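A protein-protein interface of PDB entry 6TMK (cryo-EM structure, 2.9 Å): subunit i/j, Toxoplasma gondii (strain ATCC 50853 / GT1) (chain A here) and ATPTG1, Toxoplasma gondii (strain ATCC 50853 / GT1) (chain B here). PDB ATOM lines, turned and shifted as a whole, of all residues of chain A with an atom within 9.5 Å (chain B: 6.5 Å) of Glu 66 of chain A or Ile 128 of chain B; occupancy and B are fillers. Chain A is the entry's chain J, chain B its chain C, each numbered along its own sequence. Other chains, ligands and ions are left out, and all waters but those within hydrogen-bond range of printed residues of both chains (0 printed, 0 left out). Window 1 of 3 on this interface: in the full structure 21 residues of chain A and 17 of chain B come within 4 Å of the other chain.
The backbone NH (N) of Gln 126 of chain B sits at hydrogen-bond distance from the backbone carbonyl oxygen (O) of Pro 67 of chain A, 3.0 Å away. OE1 of Gln 126 of chain B lies close to O of Pro 68 of chain A, at 3.3 Å. The side-chain carboxylate of Glu 66 of chain A sits close to the backbone carbonyl oxygen of Gln 126 of chain B (2.9 Å).
Of the 9 printed residues of chain B, 3 touch a printed residue of chain A. Printed residues of chain B that touch a printed residue of chain A: Phe 125, Gln 126 and Ile 128. Of the 8 printed residues of chain A, 3 touch a printed residue of chain B. Hydrophobic or aromatic side chains of chain A within 4 Å of the printed part of chain B: Pro 67. Among the printed residues, 6 pairs touch across the chains.
NE1 of Trp 63 of chain A lies close to OE1 of Glu 66 of chain A.
CG of Glu 66 of chain A touches CB of Phe 125 of chain B (3.8 Å). Ile 128 of chain B touches Glu 66 of chain A (CG2 to OE1, 3.5 Å). Phe 125 of chain B touches Pro 67 of chain A (CA to O, 3.3 Å).
Printed residues of chain B within 4 Å of Glu 66 of chain A: Phe 125, Gln 126 and Ile 128. Printed residues of chain B within 4 Å of Pro 67 of chain A: Phe 125 (3.3 Å) and Gln 126 (3.0 Å). Of the printed residues of chain B, Pro 68 of chain A touches Gln 126 (3.3 Å). No residue of chain A comes within 4 Å of Ser 127 of chain B. Of the printed residues of chain A, Ile 128 of chain B touches Glu 66 (3.5 Å). No residue of chain A comes within 4 Å of Ser 129 of chain B. The nearest residue of chain B that does not touch Glu 66 of chain A is Ser 127 of chain B (4.3 Å).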
ATOM      1  N   LEU A  62      14.326 -11.273 -26.828  1.00  0.00           N
ATOM      2  CA  LEU A  62      14.442  -9.951 -26.250  1.00  0.00           C
ATOM      3  C   LEU A  62      14.962 -10.034 -24.821  1.00  0.00           C
ATOM      4  O   LEU A  62      14.849 -11.058 -24.143  1.00  0.00           O
ATOM      5  CB  LEU A  62      13.091  -9.244 -26.259  1.00  0.00           C
ATOM      6  CG  LEU A  62      12.521  -8.805 -27.598  1.00  0.00           C
ATOM      7  CD1 LEU A  62      11.113  -8.374 -27.381  1.00  0.00           C
ATOM      8  CD2 LEU A  62      13.319  -7.666 -28.191  1.00  0.00           C
ATOM      9  N   TRP A  63      15.541  -8.931 -24.368  1.00  0.00           N
ATOM     10  CA  TRP A  63      16.026  -8.814 -23.002  1.00  0.00           C
ATOM     11  C   TRP A  63      14.922  -8.216 -22.143  1.00  0.00           C
ATOM     12  O   TRP A  63      14.487  -7.085 -22.381  1.00  0.00           O
ATOM     13  CB  TRP A  63      17.289  -7.960 -22.935  1.00  0.00           C
ATOM     14  CG  TRP A  63      18.172  -8.308 -21.802  1.00  0.00           C
ATOM     15  CD1 TRP A  63      18.387  -7.557 -20.693  1.00  0.00           C
ATOM     16  CD2 TRP A  63      18.955  -9.492 -21.642  1.00  0.00           C
ATOM     17  NE1 TRP A  63      19.256  -8.194 -19.850  1.00  0.00           N
ATOM     18  CE2 TRP A  63      19.621  -9.387 -20.411  1.00  0.00           C
ATOM     19  CE3 TRP A  63      19.161 -10.631 -22.421  1.00  0.00           C
ATOM     20  CZ2 TRP A  63      20.473 -10.370 -19.940  1.00  0.00           C
ATOM     21  CZ3 TRP A  63      20.010 -11.606 -21.951  1.00  0.00           C
ATOM     22  CH2 TRP A  63      20.654 -11.471 -20.724  1.00  0.00           C
ATOM     23  N   VAL A  64      14.463  -8.982 -21.152  1.00  0.00           N
ATOM     24  CA  VAL A  64      13.346  -8.577 -20.311  1.00  0.00           C
ATOM     25  C   VAL A  64      13.630  -8.771 -18.830  1.00  0.00           C
ATOM     26  O   VAL A  64      12.803  -8.393 -18.002  1.00  0.00           O
ATOM     27  CB  VAL A  64      12.053  -9.319 -20.707  1.00  0.00           C
ATOM     28  CG1 VAL A  64      11.754  -9.110 -22.166  1.00  0.00           C
ATOM     29  CG2 VAL A  64      12.160 -10.788 -20.424  1.00  0.00           C
ATOM     30  N   VAL A  65      14.781  -9.338 -18.467  1.00  0.00           N
ATOM     31  CA  VAL A  65      15.060  -9.618 -17.064  1.00  0.00           C
ATOM     32  C   VAL A  65      15.286  -8.322 -16.306  1.00  0.00           C
ATOM     33  O   VAL A  65      14.802  -8.146 -15.182  1.00  0.00           O
ATOM     34  CB  VAL A  65      16.264 -10.564 -16.936  1.00  0.00           C
ATOM     35  CG1 VAL A  65      16.670 -10.703 -15.498  1.00  0.00           C
ATOM     36  CG2 VAL A  65      15.900 -11.896 -17.467  1.00  0.00           C
ATOM     37  N   GLU A  66      16.036  -7.407 -16.901  1.00  0.00           N
ATOM     38  CA  GLU A  66      16.282  -6.100 -16.339  1.00  0.00           C
ATOM     39  C   GLU A  66      15.589  -5.069 -17.205  1.00  0.00           C
ATOM     40  O   GLU A  66      15.713  -5.126 -18.434  1.00  0.00           O
ATOM     41  CB  GLU A  66      17.780  -5.810 -16.261  1.00  0.00           C
ATOM     42  CG  GLU A  66      18.488  -5.827 -17.586  1.00  0.00           C
ATOM     43  CD  GLU A  66      19.970  -6.101 -17.449  1.00  0.00           C
ATOM     44  OE1 GLU A  66      20.335  -7.071 -16.754  1.00  0.00           O
ATOM     45  OE2 GLU A  66      20.774  -5.348 -18.037  1.00  0.00           O
ATOM     46  N   PRO A  67      14.850  -4.132 -16.628  1.00  0.00           N
ATOM     47  CA  PRO A  67      13.920  -3.349 -17.421  1.00  0.00           C
ATOM     48  C   PRO A  67      14.640  -2.318 -18.267  1.00  0.00           C
ATOM     49  O   PRO A  67      15.849  -2.098 -18.108  1.00  0.00           O
ATOM     50  CB  PRO A  67      13.034  -2.696 -16.357  1.00  0.00           C
ATOM     51  CG  PRO A  67      13.928  -2.528 -15.202  1.00  0.00           C
ATOM     52  CD  PRO A  67      14.869  -3.697 -15.223  1.00  0.00           C
ATOM     53  N   PRO A  68      13.930  -1.665 -19.176  1.00  0.00           N
ATOM     54  CA  PRO A  68      14.553  -0.649 -20.020  1.00  0.00           C
ATOM     55  C   PRO A  68      14.749   0.677 -19.307  1.00  0.00           C
ATOM     56  O   PRO A  68      14.075   1.007 -18.331  1.00  0.00           O
ATOM     57  CB  PRO A  68      13.559  -0.501 -21.174  1.00  0.00           C
ATOM     58  CG  PRO A  68      12.272  -0.885 -20.604  1.00  0.00           C
ATOM     59  CD  PRO A  68      12.547  -1.941 -19.588  1.00  0.00           C
ATOM     60  N   ASN A  69      15.702   1.440 -19.827  1.00  0.00           N
ATOM     61  CA  ASN A  69      15.981   2.794 -19.375  1.00  0.00           C
ATOM     62  C   ASN A  69      15.748   3.723 -20.559  1.00  0.00           C
ATOM     63  O   ASN A  69      16.645   3.943 -21.375  1.00  0.00           O
ATOM     64  CB  ASN A  69      17.387   2.889 -18.850  1.00  0.00           C
ATOM     65  CG  ASN A  69      17.642   4.155 -18.091  1.00  0.00           C
ATOM     66  OD1 ASN A  69      16.807   5.053 -18.045  1.00  0.00           O
ATOM     67  ND2 ASN A  69      18.814   4.240 -17.492  1.00  0.00           N
ATOM     68  N   PHE B 125      19.330  -0.580 -20.767  1.00  0.00           N
ATOM     69  CA  PHE B 125      18.632  -1.282 -19.709  1.00  0.00           C
ATOM     70  C   PHE B 125      19.300  -0.968 -18.384  1.00  0.00           C
ATOM     71  O   PHE B 125      20.464  -0.569 -18.328  1.00  0.00           O
ATOM     72  CB  PHE B 125      18.624  -2.800 -19.924  1.00  0.00           C
ATOM     73  CG  PHE B 125      18.287  -3.216 -21.313  1.00  0.00           C
ATOM     74  CD1 PHE B 125      16.975  -3.381 -21.696  1.00  0.00           C
ATOM     75  CD2 PHE B 125      19.279  -3.448 -22.237  1.00  0.00           C
ATOM     76  CE1 PHE B 125      16.662  -3.762 -22.963  1.00  0.00           C
ATOM     77  CE2 PHE B 125      18.968  -3.828 -23.508  1.00  0.00           C
ATOM     78  CZ  PHE B 125      17.657  -3.986 -23.874  1.00  0.00           C
ATOM     79  N   GLN B 126      18.536  -1.130 -17.312  1.00  0.00           N
ATOM     80  CA  GLN B 126      19.112  -1.051 -15.986  1.00  0.00           C
ATOM     81  C   GLN B 126      19.927  -2.308 -15.697  1.00  0.00           C
ATOM     82  O   GLN B 126      19.706  -3.372 -16.279  1.00  0.00           O
ATOM     83  CB  GLN B 126      18.018  -0.861 -14.946  1.00  0.00           C
ATOM     84  CG  GLN B 126      17.416   0.529 -14.966  1.00  0.00           C
ATOM     85  CD  GLN B 126      16.002   0.573 -14.445  1.00  0.00           C
ATOM     86  OE1 GLN B 126      15.063   0.857 -15.187  1.00  0.00           O
ATOM     87  NE2 GLN B 126      15.841   0.306 -13.159  1.00  0.00           N
ATOM     88  N   SER B 127      20.882  -2.177 -14.788  1.00  0.00           N
ATOM     89  CA  SER B 127      21.849  -3.232 -14.507  1.00  0.00           C
ATOM     90  C   SER B 127      21.381  -3.966 -13.258  1.00  0.00           C
ATOM     91  O   SER B 127      21.620  -3.522 -12.132  1.00  0.00           O
ATOM     92  CB  SER B 127      23.251  -2.665 -14.332  1.00  0.00           C
ATOM     93  OG  SER B 127      23.675  -1.996 -15.502  1.00  0.00           O
ATOM     94  N   ILE B 128      20.719  -5.105 -13.462  1.00  0.00           N
ATOM     95  CA  ILE B 128      20.315  -5.915 -12.325  1.00  0.00           C
ATOM     96  C   ILE B 128      21.537  -6.516 -11.656  1.00  0.00           C
ATOM     97  O   ILE B 128      21.520  -6.787 -10.454  1.00  0.00           O
ATOM     98  CB  ILE B 128      19.304  -6.994 -12.750  1.00  0.00           C
ATOM     99  CG1 ILE B 128      18.520  -7.477 -11.532  1.00  0.00           C
ATOM    100  CG2 ILE B 128      20.003  -8.159 -13.401  1.00  0.00           C
ATOM    101  CD1 ILE B 128      17.457  -8.489 -11.852  1.00  0.00           C
ATOM    102  N   SER B 129      22.621  -6.713 -12.403  1.00  0.00           N
ATOM    103  CA  SER B 129      23.849  -7.210 -11.796  1.00  0.00           C
ATOM    104  C   SER B 129      24.402  -6.202 -10.800  1.00  0.00           C
ATOM    105  O   SER B 129      24.793  -6.560  -9.684  1.00  0.00           O
ATOM    106  CB  SER B 129      24.878  -7.509 -12.881  1.00  0.00           C
ATOM    107  OG  SER B 129      24.347  -8.379 -13.860  1.00  0.00           O
ATOM    108  N   VAL B 130      24.438  -4.929 -11.190  1.00  0.00           N
ATOM    109  CA  VAL B 130      24.947  -3.894 -10.299  1.00  0.00           C
ATOM    110  C   VAL B 130      23.994  -3.686  -9.133  1.00  0.00           C
ATOM    111  O   VAL B 130      24.422  -3.480  -7.992  1.00  0.00           O
ATOM    112  CB  VAL B 130      25.175  -2.592 -11.084  1.00  0.00           C
ATOM    113  CG1 VAL B 130      25.292  -1.420 -10.143  1.00  0.00           C
ATOM    114  CG2 VAL B 130      26.403  -2.712 -11.939  1.00  0.00           C
ATOM    115  N   TYR B 131      22.691  -3.730  -9.401  1.00  0.00           N
ATOM    116  CA  TYR B 131      21.707  -3.678  -8.328  1.00  0.00           C
ATOM    117  C   TYR B 131      21.962  -4.780  -7.310  1.00  0.00           C
ATOM    118  O   TYR B 131      22.018  -4.527  -6.103  1.00  0.00           O
ATOM    119  CB  TYR B 131      20.307  -3.783  -8.925  1.00  0.00           C
ATOM    120  CG  TYR B 131      19.174  -3.769  -7.933  1.00  0.00           C
ATOM    121  CD1 TYR B 131      17.949  -4.302  -8.271  1.00  0.00           C
ATOM    122  CD2 TYR B 131      19.318  -3.217  -6.673  1.00  0.00           C
ATOM    123  CE1 TYR B 131      16.906  -4.299  -7.389  1.00  0.00           C
ATOM    124  CE2 TYR B 131      18.278  -3.214  -5.782  1.00  0.00           C
ATOM    125  CZ  TYR B 131      17.074  -3.758  -6.147  1.00  0.00           C
ATOM    126  OH  TYR B 131      16.016  -3.763  -5.275  1.00  0.00           O
ATOM    127  N   LEU B 132      22.140  -6.008  -7.788  1.00  0.00           N
ATOM    128  CA  LEU B 132      22.381  -7.144  -6.912  1.00  0.00           C
ATOM    129  C   LEU B 132      23.652  -6.947  -6.105  1.00  0.00           C
ATOM    130  O   LEU B 132      23.669  -7.161  -4.890  1.00  0.00           O
ATOM    131  CB  LEU B 132      22.464  -8.415  -7.751  1.00  0.00           C
ATOM    132  CG  LEU B 132      22.580  -9.751  -7.028  1.00  0.00           C
ATOM    133  CD1 LEU B 132      21.321 -10.064  -6.268  1.00  0.00           C
ATOM    134  CD2 LEU B 132      22.871 -10.829  -8.031  1.00  0.00           C
ATOM    135  N   ALA B 133      24.737  -6.557  -6.770  1.00  0.00           N
ATOM    136  CA  ALA B 133      26.014  -6.413  -6.084  1.00  0.00           C
ATOM    137  C   ALA B 133      25.932  -5.345  -5.003  1.00  0.00           C
ATOM    138  O   ALA B 133      26.347  -5.568  -3.860  1.00  0.00           O
ATOM    139  CB  ALA B 133      27.112  -6.075  -7.087  1.00  0.00           C
